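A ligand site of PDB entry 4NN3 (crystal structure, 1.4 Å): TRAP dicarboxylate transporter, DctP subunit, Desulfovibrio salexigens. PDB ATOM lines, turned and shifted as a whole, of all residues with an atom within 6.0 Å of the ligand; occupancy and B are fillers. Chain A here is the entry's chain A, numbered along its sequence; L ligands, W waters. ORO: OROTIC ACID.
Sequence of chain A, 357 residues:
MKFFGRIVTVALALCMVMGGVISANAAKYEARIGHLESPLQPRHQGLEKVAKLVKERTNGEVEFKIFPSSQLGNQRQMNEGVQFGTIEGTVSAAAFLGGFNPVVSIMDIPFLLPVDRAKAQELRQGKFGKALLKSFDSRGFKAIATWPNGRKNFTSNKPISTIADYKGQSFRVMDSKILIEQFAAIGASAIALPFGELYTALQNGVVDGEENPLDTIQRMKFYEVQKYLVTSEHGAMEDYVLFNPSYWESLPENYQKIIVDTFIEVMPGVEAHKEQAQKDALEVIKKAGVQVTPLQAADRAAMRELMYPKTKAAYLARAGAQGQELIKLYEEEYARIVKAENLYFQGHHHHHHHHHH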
ATOM      1  N   LEU A  36      13.025  -1.062  -3.146  1.00  0.00           N
ATOM      2  CA  LEU A  36      13.255  -2.499  -3.238  1.00  0.00           C
ATOM      3  C   LEU A  36      12.034  -3.324  -3.595  1.00  0.00           C
ATOM      4  O   LEU A  36      12.175  -4.474  -4.022  1.00  0.00           O
ATOM      5  CB  LEU A  36      13.722  -3.019  -1.895  1.00  0.00           C
ATOM      6  CG  LEU A  36      15.111  -2.709  -1.378  1.00  0.00           C
ATOM      7  CD1 LEU A  36      15.318  -3.397  -0.027  1.00  0.00           C
ATOM      8  CD2 LEU A  36      16.209  -3.063  -2.370  1.00  0.00           C
ATOM      9  N   GLU A  37      10.859  -2.781  -3.354  1.00  0.00           N
ATOM     10  CA  GLU A  37       9.635  -3.589  -3.316  1.00  0.00           C
ATOM     11  C   GLU A  37       8.990  -3.817  -4.683  1.00  0.00           C
ATOM     12  O   GLU A  37       9.229  -3.095  -5.646  1.00  0.00           O
ATOM     13  CB  GLU A  37       8.610  -2.977  -2.349  1.00  0.00           C
ATOM     14  CG  GLU A  37       8.859  -3.242  -0.865  1.00  0.00           C
ATOM     15  CD  GLU A  37       7.873  -2.527   0.002  1.00  0.00           C
ATOM     16  OE1 GLU A  37       6.859  -2.037  -0.546  1.00  0.00           O
ATOM     17  OE2 GLU A  37       8.097  -2.455   1.233  1.00  0.00           O
ATOM     18  N   GLN A  41       2.818  -3.333  -4.412  1.00  0.00           N
ATOM     19  CA  GLN A  41       2.592  -3.145  -2.983  1.00  0.00           C
ATOM     20  C   GLN A  41       2.264  -1.694  -2.650  1.00  0.00           C
ATOM     21  O   GLN A  41       2.411  -0.800  -3.492  1.00  0.00           O
ATOM     22  CB  GLN A  41       3.770  -3.672  -2.157  1.00  0.00           C
ATOM     23  CG  GLN A  41       3.875  -5.200  -2.187  1.00  0.00           C
ATOM     24  CD  GLN A  41       5.032  -5.691  -1.355  1.00  0.00           C
ATOM     25  OE1 GLN A  41       6.070  -6.070  -1.888  1.00  0.00           O
ATOM     26  NE2 GLN A  41       4.881  -5.649  -0.050  1.00  0.00           N
ATOM     27  N   ARG A  43       3.494   0.824  -0.793  1.00  0.00           N
ATOM     28  CA  ARG A  43       4.490   1.881  -0.899  1.00  0.00           C
ATOM     29  C   ARG A  43       4.567   2.400  -2.338  1.00  0.00           C
ATOM     30  O   ARG A  43       4.405   3.581  -2.577  1.00  0.00           O
ATOM     31  CB  ARG A  43       5.856   1.424  -0.405  1.00  0.00           C
ATOM     32  CG  ARG A  43       6.956   2.446  -0.632  1.00  0.00           C
ATOM     33  CD  ARG A  43       8.256   1.764  -0.805  1.00  0.00           C
ATOM     34  NE  ARG A  43       8.818   1.288   0.459  1.00  0.00           N
ATOM     35  CZ  ARG A  43       9.844   0.458   0.535  1.00  0.00           C
ATOM     36  NH1 ARG A  43      10.342   0.102   1.711  1.00  0.00           N
ATOM     37  NH2 ARG A  43      10.348  -0.088  -0.553  1.00  0.00           N
ATOM     38  N   GLN A  75      19.767  -2.077  -1.701  1.00  0.00           N
ATOM     39  CA  GLN A  75      19.492  -0.873  -0.931  1.00  0.00           C
ATOM     40  C   GLN A  75      20.750  -0.143  -0.587  1.00  0.00           C
ATOM     41  O   GLN A  75      20.745   1.083  -0.542  1.00  0.00           O
ATOM     42  CB  GLN A  75      18.721  -1.186   0.348  1.00  0.00           C
ATOM     43  CG  GLN A  75      18.209   0.074   1.034  1.00  0.00           C
ATOM     44  CD  GLN A  75      17.133   0.767   0.207  1.00  0.00           C
ATOM     45  OE1 GLN A  75      16.056   0.190  -0.006  1.00  0.00           O
ATOM     46  NE2 GLN A  75      17.385   2.004  -0.212  1.00  0.00           N
ATOM     47  N   VAL A  91      13.266   5.435  -1.223  1.00  0.00           N
ATOM     48  CA  VAL A  91      12.440   5.162  -0.051  1.00  0.00           C
ATOM     49  C   VAL A  91      12.962   3.875   0.528  1.00  0.00           C
ATOM     50  O   VAL A  91      12.774   2.803  -0.056  1.00  0.00           O
ATOM     51  CB  VAL A  91      10.948   5.053  -0.395  1.00  0.00           C
ATOM     52  CG1 VAL A  91      10.111   4.818   0.882  1.00  0.00           C
ATOM     53  CG2 VAL A  91      10.505   6.308  -1.097  1.00  0.00           C
ATOM     54  N   SER A  92      13.647   3.987   1.670  1.00  0.00           N
ATOM     55  CA  SER A  92      14.328   2.863   2.328  1.00  0.00           C
ATOM     56  C   SER A  92      13.701   2.542   3.677  1.00  0.00           C
ATOM     57  O   SER A  92      13.345   3.434   4.448  1.00  0.00           O
ATOM     58  CB  SER A  92      15.798   3.220   2.565  1.00  0.00           C
ATOM     59  OG  SER A  92      16.549   2.155   3.138  1.00  0.00           O
ATOM     60  N   ALA A  93      13.612   1.261   3.988  1.00  0.00           N
ATOM     61  CA  ALA A  93      13.328   0.878   5.346  1.00  0.00           C
ATOM     62  C   ALA A  93      14.457   1.398   6.245  1.00  0.00           C
ATOM     63  O   ALA A  93      15.627   1.451   5.873  1.00  0.00           O
ATOM     64  CB  ALA A  93      13.268  -0.609   5.437  1.00  0.00           C
ATOM     65  N   PHE A  96      17.923  -0.549   6.874  1.00  0.00           N
ATOM     66  CA  PHE A  96      19.096  -0.472   6.000  1.00  0.00           C
ATOM     67  C   PHE A  96      19.915   0.809   6.202  1.00  0.00           C
ATOM     68  O   PHE A  96      20.927   0.986   5.539  1.00  0.00           O
ATOM     69  CB  PHE A  96      18.662  -0.549   4.525  1.00  0.00           C
ATOM     70  CG  PHE A  96      18.235  -1.929   4.062  1.00  0.00           C
ATOM     71  CD1 PHE A  96      19.180  -2.870   3.720  1.00  0.00           C
ATOM     72  CD2 PHE A  96      16.884  -2.264   3.928  1.00  0.00           C
ATOM     73  CE1 PHE A  96      18.797  -4.123   3.261  1.00  0.00           C
ATOM     74  CE2 PHE A  96      16.515  -3.500   3.468  1.00  0.00           C
ATOM     75  CZ  PHE A  96      17.473  -4.428   3.139  1.00  0.00           C
ATOM     76  N   ASN A 149       5.157   1.190   7.128  1.00  0.00           N
ATOM     77  CA  ASN A 149       5.183   0.222   6.040  1.00  0.00           C
ATOM     78  C   ASN A 149       5.097  -1.216   6.546  1.00  0.00           C
ATOM     79  O   ASN A 149       5.835  -2.098   6.118  1.00  0.00           O
ATOM     80  CB  ASN A 149       6.414   0.414   5.167  1.00  0.00           C
ATOM     81  CG  ASN A 149       6.357  -0.371   3.895  1.00  0.00           C
ATOM     82  OD1 ASN A 149       5.270  -0.680   3.369  1.00  0.00           O
ATOM     83  ND2 ASN A 149       7.528  -0.686   3.352  1.00  0.00           N
ATOM     84  N   ARG A 172      17.643 -14.699   7.886  1.00  0.00           N
ATOM     85  CA  ARG A 172      18.086 -13.528   7.151  1.00  0.00           C
ATOM     86  C   ARG A 172      17.460 -12.287   7.764  1.00  0.00           C
ATOM     87  O   ARG A 172      16.280 -12.272   8.115  1.00  0.00           O
ATOM     88  CB  ARG A 172      17.685 -13.645   5.677  1.00  0.00           C
ATOM     89  CG  ARG A 172      18.029 -12.395   4.839  1.00  0.00           C
ATOM     90  CD  ARG A 172      16.889 -11.387   4.869  1.00  0.00           C
ATOM     91  NE  ARG A 172      17.147 -10.249   3.982  1.00  0.00           N
ATOM     92  CZ  ARG A 172      16.293  -9.241   3.815  1.00  0.00           C
ATOM     93  NH1 ARG A 172      15.120  -9.247   4.457  1.00  0.00           N
ATOM     94  NH2 ARG A 172      16.589  -8.236   3.008  1.00  0.00           N
ATOM     95  N   MET A 174      17.468  -7.749   7.178  1.00  0.00           N
ATOM     96  CA  MET A 174      17.904  -6.520   6.539  1.00  0.00           C
ATOM     97  C   MET A 174      19.226  -6.104   7.214  1.00  0.00           C
ATOM     98  O   MET A 174      19.612  -6.625   8.236  1.00  0.00           O
ATOM     99  CB  MET A 174      16.849  -5.438   6.667  1.00  0.00           C
ATOM    100  CG  MET A 174      15.547  -5.762   5.937  1.00  0.00           C
ATOM    101  SD  MET A 174      14.249  -4.511   6.158  1.00  0.00           S
ATOM    102  CE  MET A 174      13.732  -4.875   7.821  1.00  0.00           C
ATOM    103  N   LEU A 193      21.406 -10.368   4.173  1.00  0.00           N
ATOM    104  CA  LEU A 193      21.423 -10.742   2.762  1.00  0.00           C
ATOM    105  C   LEU A 193      20.570  -9.704   2.035  1.00  0.00           C
ATOM    106  O   LEU A 193      19.543  -9.265   2.565  1.00  0.00           O
ATOM    107  CB  LEU A 193      20.853 -12.143   2.503  1.00  0.00           C
ATOM    108  CG  LEU A 193      21.328 -13.329   3.360  1.00  0.00           C
ATOM    109  CD1 LEU A 193      20.537 -14.594   3.026  1.00  0.00           C
ATOM    110  CD2 LEU A 193      22.825 -13.561   3.179  1.00  0.00           C
ATOM    111  N   PRO A 194      20.979  -9.327   0.811  1.00  0.00           N
ATOM    112  CA  PRO A 194      20.147  -8.386   0.055  1.00  0.00           C
ATOM    113  C   PRO A 194      18.742  -8.936  -0.262  1.00  0.00           C
ATOM    114  O   PRO A 194      18.571 -10.113  -0.540  1.00  0.00           O
ATOM    115  CB  PRO A 194      20.935  -8.174  -1.250  1.00  0.00           C
ATOM    116  CG  PRO A 194      22.325  -8.644  -0.956  1.00  0.00           C
ATOM    117  CD  PRO A 194      22.196  -9.708   0.080  1.00  0.00           C
ATOM    118  N   PHE A 195      17.743  -8.071  -0.236  1.00  0.00           N
ATOM    119  CA  PHE A 195      16.362  -8.462  -0.485  1.00  0.00           C
ATOM    120  C   PHE A 195      16.155  -9.216  -1.799  1.00  0.00           C
ATOM    121  O   PHE A 195      15.452 -10.207  -1.849  1.00  0.00           O
ATOM    122  CB  PHE A 195      15.514  -7.190  -0.433  1.00  0.00           C
ATOM    123  CG  PHE A 195      14.031  -7.397  -0.470  1.00  0.00           C
ATOM    124  CD1 PHE A 195      13.406  -8.185   0.482  1.00  0.00           C
ATOM    125  CD2 PHE A 195      13.262  -6.764  -1.411  1.00  0.00           C
ATOM    126  CE1 PHE A 195      12.007  -8.344   0.484  1.00  0.00           C
ATOM    127  CE2 PHE A 195      11.886  -6.925  -1.429  1.00  0.00           C
ATOM    128  CZ  PHE A 195      11.247  -7.714  -0.471  1.00  0.00           C
ATOM    129  N   LEU A 198      16.801 -12.846  -1.524  1.00  0.00           N
ATOM    130  CA  LEU A 198      16.178 -13.557  -0.396  1.00  0.00           C
ATOM    131  C   LEU A 198      15.397 -14.817  -0.816  1.00  0.00           C
ATOM    132  O   LEU A 198      15.549 -15.847  -0.206  1.00  0.00           O
ATOM    133  CB  LEU A 198      15.309 -12.609   0.438  1.00  0.00           C
ATOM    134  CG  LEU A 198      14.612 -13.216   1.672  1.00  0.00           C
ATOM    135  CD1 LEU A 198      15.591 -14.030   2.549  1.00  0.00           C
ATOM    136  CD2 LEU A 198      13.944 -12.140   2.501  1.00  0.00           C
ATOM    137  N   GLU A 210      13.195 -15.948   7.873  1.00  0.00           N
ATOM    138  CA  GLU A 210      13.302 -14.514   7.635  1.00  0.00           C
ATOM    139  C   GLU A 210      12.149 -13.828   8.375  1.00  0.00           C
ATOM    140  O   GLU A 210      11.419 -14.498   9.108  1.00  0.00           O
ATOM    141  CB  GLU A 210      13.301 -14.202   6.123  1.00  0.00           C
ATOM    142  CG  GLU A 210      12.042 -14.612   5.362  1.00  0.00           C
ATOM    143  CD  GLU A 210      10.872 -13.616   5.466  1.00  0.00           C
ATOM    144  OE1 GLU A 210       9.760 -13.998   5.950  1.00  0.00           O
ATOM    145  OE2 GLU A 210      11.043 -12.457   5.030  1.00  0.00           O
ATOM    146  N   GLU A 211      12.017 -12.515   8.233  1.00  0.00           N
ATOM    147  CA  GLU A 211      10.938 -11.762   8.883  1.00  0.00           C
ATOM    148  C   GLU A 211      10.460 -10.678   7.940  1.00  0.00           C
ATOM    149  O   GLU A 211      11.283  -9.987   7.321  1.00  0.00           O
ATOM    150  CB  GLU A 211      11.413 -11.111  10.206  1.00  0.00           C
ATOM    151  CG  GLU A 211      12.710 -10.300  10.069  1.00  0.00           C
ATOM    152  CD  GLU A 211      12.979  -9.314  11.202  1.00  0.00           C
ATOM    153  OE1 GLU A 211      12.390  -9.393  12.296  1.00  0.00           O
ATOM    154  OE2 GLU A 211      13.793  -8.379  10.964  1.00  0.00           O
ATOM    155  N   ASN A 212       9.160 -10.492   7.818  1.00  0.00           N
ATOM    156  CA  ASN A 212       8.607  -9.514   6.888  1.00  0.00           C
ATOM    157  C   ASN A 212       7.109  -9.378   7.095  1.00  0.00           C
ATOM    158  O   ASN A 212       6.471 -10.255   7.719  1.00  0.00           O
ATOM    159  CB  ASN A 212       8.878  -9.927   5.457  1.00  0.00           C
ATOM    160  CG  ASN A 212       9.947  -9.049   4.782  1.00  0.00           C
ATOM    161  OD1 ASN A 212       9.862  -7.825   4.837  1.00  0.00           O
ATOM    162  ND2 ASN A 212      10.972  -9.667   4.160  1.00  0.00           N
ATOM    163  N   PRO A 213       6.535  -8.284   6.598  1.00  0.00           N
ATOM    164  CA  PRO A 213       5.073  -8.161   6.601  1.00  0.00           C
ATOM    165  C   PRO A 213       4.466  -9.245   5.712  1.00  0.00           C
ATOM    166  O   PRO A 213       5.092  -9.724   4.755  1.00  0.00           O
ATOM    167  CB  PRO A 213       4.815  -6.751   6.040  1.00  0.00           C
ATOM    168  CG  PRO A 213       6.074  -5.987   6.371  1.00  0.00           C
ATOM    169  CD  PRO A 213       7.186  -7.027   6.181  1.00  0.00           C
ATOM    170  N   THR A 216       4.447  -8.586   1.870  1.00  0.00           N
ATOM    171  CA  THR A 216       5.777  -8.804   1.293  1.00  0.00           C
ATOM    172  C   THR A 216       6.054 -10.297   1.089  1.00  0.00           C
ATOM    173  O   THR A 216       6.485 -10.699   0.023  1.00  0.00           O
ATOM    174  CB  THR A 216       6.855  -8.153   2.153  1.00  0.00           C
ATOM    175  OG1 THR A 216       6.626  -6.739   2.173  1.00  0.00           O
ATOM    176  CG2 THR A 216       8.231  -8.427   1.590  1.00  0.00           C
ATOM    177  N   MET A 237       8.490  -2.243  10.119  1.00  0.00           N
ATOM    178  CA  MET A 237       9.094  -1.893   8.826  1.00  0.00           C
ATOM    179  C   MET A 237       8.730  -0.424   8.583  1.00  0.00           C
ATOM    180  O   MET A 237       7.561  -0.086   8.328  1.00  0.00           O
ATOM    181  CB  MET A 237       8.499  -2.771   7.729  1.00  0.00           C
ATOM    182  CG  MET A 237       9.163  -2.635   6.343  1.00  0.00           C
ATOM    183  SD  MET A 237      10.841  -3.251   6.254  1.00  0.00           S
ATOM    184  CE  MET A 237      10.539  -5.012   6.387  1.00  0.00           C
ATOM    185  N   ASP A 239       9.390   3.208   6.687  1.00  0.00           N
ATOM    186  CA  ASP A 239       9.909   3.808   5.449  1.00  0.00           C
ATOM    187  C   ASP A 239      10.397   5.241   5.661  1.00  0.00           C
ATOM    188  O   ASP A 239       9.691   6.064   6.270  1.00  0.00           O
ATOM    189  CB  ASP A 239       8.825   3.839   4.371  1.00  0.00           C
ATOM    190  CG  ASP A 239       8.677   2.536   3.628  1.00  0.00           C
ATOM    191  OD1 ASP A 239       9.421   1.570   3.938  1.00  0.00           O
ATOM    192  OD2 ASP A 239       7.795   2.459   2.749  1.00  0.00           O
ATOM    193  N   LYS A 274      -2.048  -0.853   3.108  1.00  0.00           N
ATOM    194  CA  LYS A 274      -1.055  -1.788   3.683  1.00  0.00           C
ATOM    195  C   LYS A 274      -1.709  -2.682   4.743  1.00  0.00           C
ATOM    196  O   LYS A 274      -1.500  -3.907   4.763  1.00  0.00           O
ATOM    197  CB  LYS A 274       0.133  -1.023   4.248  1.00  0.00           C
ATOM    198  CG  LYS A 274       1.293  -1.914   4.657  1.00  0.00           C
ATOM    199  CD  LYS A 274       2.030  -2.547   3.461  1.00  0.00           C
ATOM    200  CE  LYS A 274       3.334  -3.199   3.939  1.00  0.00           C
ATOM    201  NZ  LYS A 274       4.073  -3.721   2.735  1.00  0.00           N
HETATM  202  N1  ORO L   1      11.035  -5.820   3.125  1.00  0.00           N
HETATM  203  C2  ORO L   1      10.047  -4.953   2.814  1.00  0.00           C
HETATM  204  O2  ORO L   1       8.858  -5.217   3.068  1.00  0.00           O
HETATM  205  N3  ORO L   1      10.343  -3.768   2.203  1.00  0.00           N
HETATM  206  C4  ORO L   1      11.618  -3.435   1.957  1.00  0.00           C
HETATM  207  O4  ORO L   1      11.808  -2.338   1.433  1.00  0.00           O
HETATM  208  C5  ORO L   1      12.633  -4.302   2.279  1.00  0.00           C
HETATM  209  C6  ORO L   1      12.320  -5.516   2.829  1.00  0.00           C
HETATM  210  C7  ORO L   1      13.369  -6.503   3.205  1.00  0.00           C
HETATM  211  O71 ORO L   1      14.582  -6.310   2.854  1.00  0.00           O
HETATM  212  O72 ORO L   1      13.049  -7.522   3.879  1.00  0.00           O
HETATM  213  O   HOH W   1      12.839  -7.818   6.569  1.00  0.00           O
HETATM  214  O   HOH W   2      14.298  -0.867   2.174  1.00  0.00           O
HETATM  215  O   HOH W   3       6.606  -3.866   3.893  1.00  0.00           O
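Water W2 lies within hydrogen-bond range of N of Ala 93 (2.9 Å), O4 of the ligand (3.0 Å) and OE1 of Gln 75 (3.0 Å).
An oxygen (O2) of the ligand sits at hydrogen-bond distance from the side-chain hydroxyl (OG1) of Thr 216, at 2.8 Å. The side-chain carboxylate (OE2) of Glu 37 lies within hydrogen-bond range of a nitrogen (N3) of the ligand. A nitrogen (N1) of the ligand is in hydrogen-bond range of the side-chain amide oxygen (OD1) of Asn 212. NH1 of Arg 172 lies within salt-bridge range of O72 of the ligand, at 2.8 Å. An oxygen (O4) of the ligand lies within hydrogen-bond range of the guanidinium group of Arg 43 (2.9 Å).
SD of Met 174 lies close to O71 of the ligand, at 3.8 Å. Merely in contact with the ligand: Phe 195 (3.2 Å), Met 237 (3.4 Å), Phe 96 (3.5 Å), Leu 36 (3.7 Å) and Pro 213 (3.97 Å). Hydrophobic or aromatic side chains that line the ligand: Leu 36, Phe 96, Met 174, Phe 195, Pro 213 and Met 237. Of the 24 residues printed, 11 come within 4 Å of the ligand. Along chain A the residues within 4 Å of the ligand span positions 36 to 237. The nearest printed residue that does not touch the ligand is Asn 149 (4.3 Å).
OE2 of Glu 37 lies within salt-bridge range of NH1 of Arg 43. The guanidinium group (NH1) of Arg 43 sits close to the side-chain amide nitrogen (ND2) of Asn 149 (3.4 Å). The side-chain hydroxyl (OG1) of Thr 216 lies within hydrogen-bond range of the side-chain amide nitrogen (NE2) of Gln 41. ND2 of Asn 212 sits at hydrogen-bond distance from OE2 of Glu 210, 2.9 Å away. The backbone carbonyl oxygen (O) of Leu 193 lies within hydrogen-bond range of the guanidinium group (NE) of Arg 172 (3.0 Å). The side-chain carboxylate (OE2) of Glu 37 lies within hydrogen-bond range of the side-chain amide nitrogen (ND2) of Asn 149 (2.8 Å). The backbone carbonyl oxygen of Met 237 is in hydrogen-bond range of the backbone NH of Asn 149 (3.0 Å). The guanidinium group of Arg 43 lies within salt-bridge range of the side-chain carboxylate of Asp 239 (2.8 Å).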
